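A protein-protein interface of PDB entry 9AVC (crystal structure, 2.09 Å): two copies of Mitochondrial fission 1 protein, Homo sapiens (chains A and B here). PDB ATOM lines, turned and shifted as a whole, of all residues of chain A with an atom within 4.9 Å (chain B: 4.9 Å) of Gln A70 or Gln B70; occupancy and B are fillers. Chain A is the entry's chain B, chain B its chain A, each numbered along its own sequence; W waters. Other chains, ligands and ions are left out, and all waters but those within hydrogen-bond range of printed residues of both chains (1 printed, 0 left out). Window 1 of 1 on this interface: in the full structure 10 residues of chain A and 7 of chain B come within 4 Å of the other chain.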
ATOM      1  N   LEU A  62       5.304  16.349  -3.875  1.00  0.00           N
ATOM      2  CA  LEU A  62       5.592  14.935  -4.125  1.00  0.00           C
ATOM      3  C   LEU A  62       4.359  14.053  -4.217  1.00  0.00           C
ATOM      4  O   LEU A  62       4.258  13.278  -5.181  1.00  0.00           O
ATOM      5  CB  LEU A  62       6.550  14.429  -3.034  1.00  0.00           C
ATOM      6  CG  LEU A  62       7.123  13.014  -3.097  1.00  0.00           C
ATOM      7  CD1 LEU A  62       7.856  12.788  -4.398  1.00  0.00           C
ATOM      8  CD2 LEU A  62       8.053  12.766  -1.913  1.00  0.00           C
ATOM      9  N   PRO A  63       3.407  14.093  -3.282  1.00  0.00           N
ATOM     10  CA  PRO A  63       2.218  13.245  -3.427  1.00  0.00           C
ATOM     11  C   PRO A  63       1.309  13.681  -4.555  1.00  0.00           C
ATOM     12  O   PRO A  63       0.367  12.956  -4.891  1.00  0.00           O
ATOM     13  CB  PRO A  63       1.510  13.378  -2.072  1.00  0.00           C
ATOM     14  CG  PRO A  63       2.059  14.571  -1.421  1.00  0.00           C
ATOM     15  CD  PRO A  63       3.443  14.786  -1.979  1.00  0.00           C
ATOM     16  N   LYS A  64       1.549  14.839  -5.153  1.00  0.00           N
ATOM     17  CA  LYS A  64       0.661  15.345  -6.187  1.00  0.00           C
ATOM     18  C   LYS A  64       1.208  15.123  -7.590  1.00  0.00           C
ATOM     19  O   LYS A  64       0.539  15.469  -8.567  1.00  0.00           O
ATOM     20  CB  LYS A  64       0.379  16.837  -5.951  1.00  0.00           C
ATOM     21  CG  LYS A  64      -0.254  17.139  -4.584  1.00  0.00           C
ATOM     22  CD  LYS A  64      -0.926  18.516  -4.544  1.00  0.00           C
ATOM     23  CE  LYS A  64       0.081  19.637  -4.738  1.00  0.00           C
ATOM     24  NZ  LYS A  64      -0.142  20.778  -3.801  1.00  0.00           N
ATOM     25  N   GLY A  65       2.391  14.536  -7.719  1.00  0.00           N
ATOM     26  CA  GLY A  65       3.052  14.451  -8.997  1.00  0.00           C
ATOM     27  C   GLY A  65       2.805  13.146  -9.724  1.00  0.00           C
ATOM     28  O   GLY A  65       2.452  12.134  -9.131  1.00  0.00           O
ATOM     29  N   SER A  66       3.003  13.186 -11.037  1.00  0.00           N
ATOM     30  CA  SER A  66       3.036  11.965 -11.823  1.00  0.00           C
ATOM     31  C   SER A  66       4.287  11.159 -11.483  1.00  0.00           C
ATOM     32  O   SER A  66       5.222  11.654 -10.850  1.00  0.00           O
ATOM     33  CB  SER A  66       3.025  12.295 -13.303  1.00  0.00           C
ATOM     34  OG  SER A  66       4.282  12.850 -13.633  1.00  0.00           O
ATOM     35  N   LYS A  67       4.310   9.899 -11.922  1.00  0.00           N
ATOM     36  CA  LYS A  67       5.435   9.035 -11.570  1.00  0.00           C
ATOM     37  C   LYS A  67       6.762   9.616 -12.044  1.00  0.00           C
ATOM     38  O   LYS A  67       7.787   9.444 -11.371  1.00  0.00           O
ATOM     39  CB  LYS A  67       5.232   7.632 -12.146  1.00  0.00           C
ATOM     40  CG  LYS A  67       6.121   7.324 -13.336  1.00  0.00           C
ATOM     41  CD  LYS A  67       5.512   6.273 -14.251  1.00  0.00           C
ATOM     42  CE  LYS A  67       6.443   5.998 -15.422  1.00  0.00           C
ATOM     43  NZ  LYS A  67       7.535   5.054 -15.048  1.00  0.00           N
ATOM     44  N   GLU A  68       6.760  10.319 -13.177  1.00  0.00           N
ATOM     45  CA  GLU A  68       7.982  10.929 -13.690  1.00  0.00           C
ATOM     46  C   GLU A  68       8.323  12.202 -12.924  1.00  0.00           C
ATOM     47  O   GLU A  68       9.493  12.462 -12.610  1.00  0.00           O
ATOM     48  CB  GLU A  68       7.823  11.236 -15.180  1.00  0.00           C
ATOM     49  CG  GLU A  68       8.719  12.374 -15.648  1.00  0.00           C
ATOM     50  CD  GLU A  68       9.212  12.200 -17.074  1.00  0.00           C
ATOM     51  OE1 GLU A  68       9.169  11.067 -17.605  1.00  0.00           O
ATOM     52  OE2 GLU A  68       9.639  13.209 -17.665  1.00  0.00           O
ATOM     53  N   GLU A  69       7.311  13.018 -12.625  1.00  0.00           N
ATOM     54  CA  GLU A  69       7.548  14.206 -11.814  1.00  0.00           C
ATOM     55  C   GLU A  69       8.106  13.828 -10.446  1.00  0.00           C
ATOM     56  O   GLU A  69       8.997  14.504  -9.915  1.00  0.00           O
ATOM     57  CB  GLU A  69       6.251  15.004 -11.673  1.00  0.00           C
ATOM     58  CG  GLU A  69       5.864  15.799 -12.922  1.00  0.00           C
ATOM     59  CD  GLU A  69       4.411  16.262 -12.891  1.00  0.00           C
ATOM     60  OE1 GLU A  69       3.591  15.654 -12.165  1.00  0.00           O
ATOM     61  OE2 GLU A  69       4.092  17.258 -13.570  1.00  0.00           O
ATOM     62  N   GLN A  70       7.615  12.728  -9.876  1.00  0.00           N
ATOM     63  CA  GLN A  70       8.079  12.328  -8.558  1.00  0.00           C
ATOM     64  C   GLN A  70       9.554  11.968  -8.585  1.00  0.00           C
ATOM     65  O   GLN A  70      10.265  12.196  -7.604  1.00  0.00           O
ATOM     66  CB  GLN A  70       7.232  11.167  -8.057  1.00  0.00           C
ATOM     67  CG  GLN A  70       5.879  11.633  -7.545  1.00  0.00           C
ATOM     68  CD  GLN A  70       5.010  10.495  -7.060  1.00  0.00           C
ATOM     69  OE1 GLN A  70       5.248   9.325  -7.382  1.00  0.00           O
ATOM     70  NE2 GLN A  70       3.986  10.831  -6.276  1.00  0.00           N
ATOM     71  N   ARG A  71      10.031  11.434  -9.709  1.00  0.00           N
ATOM     72  CA  ARG A  71      11.456  11.164  -9.881  1.00  0.00           C
ATOM     73  C   ARG A  71      12.271  12.443  -9.843  1.00  0.00           C
ATOM     74  O   ARG A  71      13.343  12.491  -9.232  1.00  0.00           O
ATOM     75  CB  ARG A  71      11.698  10.488 -11.218  1.00  0.00           C
ATOM     76  CG  ARG A  71      11.008   9.200 -11.348  1.00  0.00           C
ATOM     77  CD  ARG A  71      11.569   8.384 -12.487  1.00  0.00           C
ATOM     78  NE  ARG A  71      11.438   6.975 -12.154  1.00  0.00           N
ATOM     79  CZ  ARG A  71      12.103   6.356 -11.187  1.00  0.00           C
ATOM     80  NH1 ARG A  71      13.096   6.947 -10.527  1.00  0.00           N
ATOM     81  NH2 ARG A  71      11.766   5.108 -10.876  1.00  0.00           N
ATOM     82  N   ASP A  72      11.806  13.467 -10.554  1.00  0.00           N
ATOM     83  CA  ASP A  72      12.453  14.766 -10.498  1.00  0.00           C
ATOM     84  C   ASP A  72      12.389  15.324  -9.094  1.00  0.00           C
ATOM     85  O   ASP A  72      13.416  15.703  -8.525  1.00  0.00           O
ATOM     86  CB  ASP A  72      11.792  15.725 -11.479  1.00  0.00           C
ATOM     87  CG  ASP A  72      11.952  15.280 -12.908  1.00  0.00           C
ATOM     88  OD1 ASP A  72      12.839  14.437 -13.174  1.00  0.00           O
ATOM     89  OD2 ASP A  72      11.174  15.757 -13.759  1.00  0.00           O
ATOM     90  N   TYR A  73      11.182  15.359  -8.511  1.00  0.00           N
ATOM     91  CA  TYR A  73      11.038  15.857  -7.151  1.00  0.00           C
ATOM     92  C   TYR A  73      12.034  15.181  -6.219  1.00  0.00           C
ATOM     93  O   TYR A  73      12.718  15.849  -5.431  1.00  0.00           O
ATOM     94  CB  TYR A  73       9.604  15.638  -6.647  1.00  0.00           C
ATOM     95  CG  TYR A  73       8.512  16.350  -7.433  1.00  0.00           C
ATOM     96  CD1 TYR A  73       8.793  17.451  -8.234  1.00  0.00           C
ATOM     97  CD2 TYR A  73       7.196  15.924  -7.355  1.00  0.00           C
ATOM     98  CE1 TYR A  73       7.779  18.104  -8.942  1.00  0.00           C
ATOM     99  CE2 TYR A  73       6.187  16.568  -8.040  1.00  0.00           C
ATOM    100  CZ  TYR A  73       6.478  17.648  -8.842  1.00  0.00           C
ATOM    101  OH  TYR A  73       5.451  18.267  -9.529  1.00  0.00           O
ATOM    102  N   VAL A  74      12.178  13.859  -6.341  1.00  0.00           N
ATOM    103  CA  VAL A  74      13.023  13.108  -5.411  1.00  0.00           C
ATOM    104  C   VAL A  74      14.489  13.495  -5.572  1.00  0.00           C
ATOM    105  O   VAL A  74      15.223  13.622  -4.585  1.00  0.00           O
ATOM    106  CB  VAL A  74      12.817  11.595  -5.615  1.00  0.00           C
ATOM    107  CG1 VAL A  74      14.019  10.827  -5.095  1.00  0.00           C
ATOM    108  CG2 VAL A  74      11.536  11.139  -4.923  1.00  0.00           C
ATOM    109  N   LEU B  62       5.937   6.491  -0.331  1.00  0.00           N
ATOM    110  CA  LEU B  62       5.225   7.450  -1.171  1.00  0.00           C
ATOM    111  C   LEU B  62       5.743   7.499  -2.607  1.00  0.00           C
ATOM    112  O   LEU B  62       4.928   7.366  -3.532  1.00  0.00           O
ATOM    113  CB  LEU B  62       5.280   8.813  -0.464  1.00  0.00           C
ATOM    114  CG  LEU B  62       4.398   9.964  -0.932  1.00  0.00           C
ATOM    115  CD1 LEU B  62       2.972   9.474  -1.070  1.00  0.00           C
ATOM    116  CD2 LEU B  62       4.492  11.138   0.059  1.00  0.00           C
ATOM    117  N   PRO B  63       7.047   7.652  -2.874  1.00  0.00           N
ATOM    118  CA  PRO B  63       7.494   7.624  -4.279  1.00  0.00           C
ATOM    119  C   PRO B  63       7.335   6.268  -4.955  1.00  0.00           C
ATOM    120  O   PRO B  63       7.291   6.213  -6.193  1.00  0.00           O
ATOM    121  CB  PRO B  63       8.976   8.023  -4.192  1.00  0.00           C
ATOM    122  CG  PRO B  63       9.122   8.721  -2.885  1.00  0.00           C
ATOM    123  CD  PRO B  63       8.129   8.076  -1.967  1.00  0.00           C
ATOM    124  N   GLY B  65       4.880   3.945  -4.816  1.00  0.00           N
ATOM    125  CA  GLY B  65       3.568   3.341  -4.961  1.00  0.00           C
ATOM    126  C   GLY B  65       2.874   3.682  -6.269  1.00  0.00           C
ATOM    127  O   GLY B  65       3.069   4.747  -6.836  1.00  0.00           O
ATOM    128  N   SER B  66       2.028   2.760  -6.733  1.00  0.00           N
ATOM    129  CA  SER B  66       1.090   3.084  -7.806  1.00  0.00           C
ATOM    130  C   SER B  66       0.154   4.201  -7.349  1.00  0.00           C
ATOM    131  O   SER B  66       0.247   4.664  -6.208  1.00  0.00           O
ATOM    132  CB  SER B  66       0.307   1.835  -8.227  1.00  0.00           C
ATOM    133  OG  SER B  66      -0.662   1.490  -7.254  1.00  0.00           O
ATOM    134  N   LYS B  67      -0.751   4.657  -8.210  1.00  0.00           N
ATOM    135  CA  LYS B  67      -1.583   5.781  -7.798  1.00  0.00           C
ATOM    136  C   LYS B  67      -2.648   5.349  -6.803  1.00  0.00           C
ATOM    137  O   LYS B  67      -2.894   6.050  -5.813  1.00  0.00           O
ATOM    138  CB  LYS B  67      -2.213   6.459  -9.007  1.00  0.00           C
ATOM    139  CG  LYS B  67      -1.674   7.859  -9.209  1.00  0.00           C
ATOM    140  CD  LYS B  67      -0.191   7.804  -9.530  1.00  0.00           C
ATOM    141  CE  LYS B  67       0.263   9.030 -10.288  1.00  0.00           C
ATOM    142  NZ  LYS B  67       1.746   9.094 -10.365  1.00  0.00           N
ATOM    143  N   GLU B  68      -3.291   4.201  -7.037  1.00  0.00           N
ATOM    144  CA  GLU B  68      -4.248   3.721  -6.052  1.00  0.00           C
ATOM    145  C   GLU B  68      -3.563   3.241  -4.784  1.00  0.00           C
ATOM    146  O   GLU B  68      -4.254   2.938  -3.803  1.00  0.00           O
ATOM    147  CB  GLU B  68      -5.126   2.605  -6.627  1.00  0.00           C
ATOM    148  CG  GLU B  68      -4.429   1.266  -6.859  1.00  0.00           C
ATOM    149  CD  GLU B  68      -3.884   1.099  -8.271  1.00  0.00           C
ATOM    150  OE1 GLU B  68      -3.829   2.098  -9.029  1.00  0.00           O
ATOM    151  OE2 GLU B  68      -3.516  -0.044  -8.622  1.00  0.00           O
ATOM    152  N   GLU B  69      -2.233   3.158  -4.785  1.00  0.00           N
ATOM    153  CA  GLU B  69      -1.481   2.913  -3.562  1.00  0.00           C
ATOM    154  C   GLU B  69      -1.176   4.221  -2.835  1.00  0.00           C
ATOM    155  O   GLU B  69      -1.354   4.306  -1.614  1.00  0.00           O
ATOM    156  CB  GLU B  69      -0.188   2.143  -3.879  1.00  0.00           C
ATOM    157  CG  GLU B  69      -0.403   0.624  -4.027  1.00  0.00           C
ATOM    158  CD  GLU B  69       0.795  -0.141  -4.611  1.00  0.00           C
ATOM    159  OE1 GLU B  69       1.851   0.470  -4.894  1.00  0.00           O
ATOM    160  OE2 GLU B  69       0.665  -1.372  -4.808  1.00  0.00           O
ATOM    161  N   GLN B  70      -0.760   5.257  -3.573  1.00  0.00           N
ATOM    162  CA  GLN B  70      -0.414   6.534  -2.949  1.00  0.00           C
ATOM    163  C   GLN B  70      -1.626   7.178  -2.282  1.00  0.00           C
ATOM    164  O   GLN B  70      -1.480   7.867  -1.274  1.00  0.00           O
ATOM    165  CB  GLN B  70       0.189   7.462  -4.008  1.00  0.00           C
ATOM    166  CG  GLN B  70       1.539   6.992  -4.513  1.00  0.00           C
ATOM    167  CD  GLN B  70       2.262   8.027  -5.361  1.00  0.00           C
ATOM    168  OE1 GLN B  70       1.820   9.169  -5.491  1.00  0.00           O
ATOM    169  NE2 GLN B  70       3.355   7.605  -5.995  1.00  0.00           N
ATOM    170  N   ARG B  71      -2.820   6.988  -2.846  1.00  0.00           N
ATOM    171  CA  ARG B  71      -4.075   7.301  -2.166  1.00  0.00           C
ATOM    172  C   ARG B  71      -4.041   6.940  -0.678  1.00  0.00           C
ATOM    173  O   ARG B  71      -4.207   7.798   0.202  1.00  0.00           O
ATOM    174  CB  ARG B  71      -5.186   6.518  -2.869  1.00  0.00           C
ATOM    175  CG  ARG B  71      -6.453   7.268  -3.118  1.00  0.00           C
ATOM    176  CD  ARG B  71      -7.304   6.470  -4.087  1.00  0.00           C
ATOM    177  NE  ARG B  71      -7.872   5.313  -3.421  1.00  0.00           N
ATOM    178  CZ  ARG B  71      -8.954   5.346  -2.657  1.00  0.00           C
ATOM    179  NH1 ARG B  71      -9.623   6.470  -2.453  1.00  0.00           N
ATOM    180  NH2 ARG B  71      -9.374   4.222  -2.088  1.00  0.00           N
ATOM    181  N   ASP B  72      -3.827   5.650  -0.396  1.00  0.00           N
ATOM    182  CA  ASP B  72      -3.770   5.183   0.989  1.00  0.00           C
ATOM    183  C   ASP B  72      -2.590   5.795   1.732  1.00  0.00           C
ATOM    184  O   ASP B  72      -2.725   6.204   2.892  1.00  0.00           O
ATOM    185  CB  ASP B  72      -3.669   3.657   1.049  1.00  0.00           C
ATOM    186  CG  ASP B  72      -4.866   2.942   0.430  1.00  0.00           C
ATOM    187  OD1 ASP B  72      -5.972   3.519   0.379  1.00  0.00           O
ATOM    188  OD2 ASP B  72      -4.709   1.758   0.049  1.00  0.00           O
ATOM    189  N   TYR B  73      -1.415   5.844   1.093  1.00  0.00           N
ATOM    190  CA  TYR B  73      -0.256   6.446   1.743  1.00  0.00           C
ATOM    191  C   TYR B  73      -0.566   7.866   2.194  1.00  0.00           C
ATOM    192  O   TYR B  73      -0.250   8.254   3.329  1.00  0.00           O
ATOM    193  CB  TYR B  73       0.954   6.479   0.812  1.00  0.00           C
ATOM    194  CG  TYR B  73       1.456   5.163   0.297  1.00  0.00           C
ATOM    195  CD1 TYR B  73       1.149   3.971   0.934  1.00  0.00           C
ATOM    196  CD2 TYR B  73       2.262   5.121  -0.840  1.00  0.00           C
ATOM    197  CE1 TYR B  73       1.620   2.767   0.446  1.00  0.00           C
ATOM    198  CE2 TYR B  73       2.746   3.927  -1.329  1.00  0.00           C
ATOM    199  CZ  TYR B  73       2.422   2.751  -0.686  1.00  0.00           C
ATOM    200  OH  TYR B  73       2.901   1.557  -1.184  1.00  0.00           O
ATOM    201  N   VAL B  74      -1.163   8.665   1.300  1.00  0.00           N
ATOM    202  CA  VAL B  74      -1.406  10.075   1.608  1.00  0.00           C
ATOM    203  C   VAL B  74      -2.435  10.190   2.723  1.00  0.00           C
ATOM    204  O   VAL B  74      -2.289  10.993   3.652  1.00  0.00           O
ATOM    205  CB  VAL B  74      -1.853  10.840   0.346  1.00  0.00           C
ATOM    206  CG1 VAL B  74      -2.333  12.224   0.711  1.00  0.00           C
ATOM    207  CG2 VAL B  74      -0.718  10.940  -0.700  1.00  0.00           C
ATOM    208  N   PHE B  75      -3.484   9.373   2.665  1.00  0.00           N
ATOM    209  CA  PHE B  75      -4.489   9.410   3.719  1.00  0.00           C
ATOM    210  C   PHE B  75      -3.881   9.062   5.074  1.00  0.00           C
ATOM    211  O   PHE B  75      -4.116   9.760   6.065  1.00  0.00           O
ATOM    212  CB  PHE B  75      -5.652   8.478   3.391  1.00  0.00           C
ATOM    213  CG  PHE B  75      -6.712   8.465   4.467  1.00  0.00           C
ATOM    214  CD1 PHE B  75      -7.517   9.572   4.679  1.00  0.00           C
ATOM    215  CD2 PHE B  75      -6.877   7.361   5.275  1.00  0.00           C
ATOM    216  CE1 PHE B  75      -8.492   9.569   5.674  1.00  0.00           C
ATOM    217  CE2 PHE B  75      -7.850   7.349   6.282  1.00  0.00           C
ATOM    218  CZ  PHE B  75      -8.654   8.462   6.475  1.00  0.00           C
HETATM  219  O   HOH W   1       2.054   9.079 -13.590  1.00  0.00           O
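NZ of Lys B67 lies close to N of Lys A67, 3.1 Å away. O of Gly A65 is in hydrogen-bond range of NZ of Lys B67 (3.4 Å). OE1 of Gln B70 lies within hydrogen-bond range of NE2 of Gln A70 (2.8 Å).
The side-chain amide nitrogen (NE2) of Gln A70 sits at hydrogen-bond distance from the backbone carbonyl oxygen (O) of Gly A65 (3.5 Å). The side-chain amide nitrogen (NE2) of Gln B70 lies within hydrogen-bond range of the backbone carbonyl oxygen (O) of Leu B62 (2.9 Å). O of Gly B65 is in hydrogen-bond range of NE2 of Gln B70 (3.0 Å). The side-chain carboxylate of Glu A69 is in hydrogen-bond range of the backbone NH of Ser A66 (2.8 Å). NE2 of Gln A70 lies within hydrogen-bond range of O of Leu A62, 2.7 Å away.
Among the printed residues, pairs that only touch across the chains: Ser A66 with Lys B67 (3.5 Å), Pro A63 with Val B74 (3.6 Å), Gln A70 with Pro B63 (3.9 Å) and Val A74 with Pro B63 (3.98 Å).
Printed residues of chain B within 4 Å of Pro A63: Val B74. Of chain B, only Pro B63 (3.9 Å) and Gln B70 (2.8 Å) come within 4 Å of Gln A70. Of the printed residues of chain B, Val A74 touches Pro B63. Gln B70 touches just one residue of chain A: Gln A70.
Hydrophobic or aromatic side chains of chain B within 4 Å of the printed part of chain A: Pro B63 and Val B74. Of the 13 printed residues of chain A, 6 touch a printed residue of chain B. Hydrophobic or aromatic side chains of chain A that line the printed part of chain B: Pro A63 and Val A74. Among the printed residues, no Asp or Glu carboxylate lies within 4 Å of a Lys or Arg side-chain nitrogen of the other chain.
Gly A65 touches Lys B67, but with the chains exchanged Lys A67 does not touch Gly B65 (6.4 Å). Lys A67 touches its own counterpart, Lys B67. Gln A70 touches Pro B63, but with the chains exchanged Pro A63 does not touch Gln B70 (4.1 Å). Gln B70 touches its own counterpart, Gln A70. Positions printed for both chains: 62, 63, 65, 66, 67, 68, 69, 70, 71, 72, 73 and 74. Of the 7 pairs that touch across the chains among the printed residues, 4 have their exchanged pair printed and touching as well.
Water W1 lies within hydrogen-bond range of N of Lys A67 (2.9 Å) and NZ of Lys B67 (3.2 Å).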
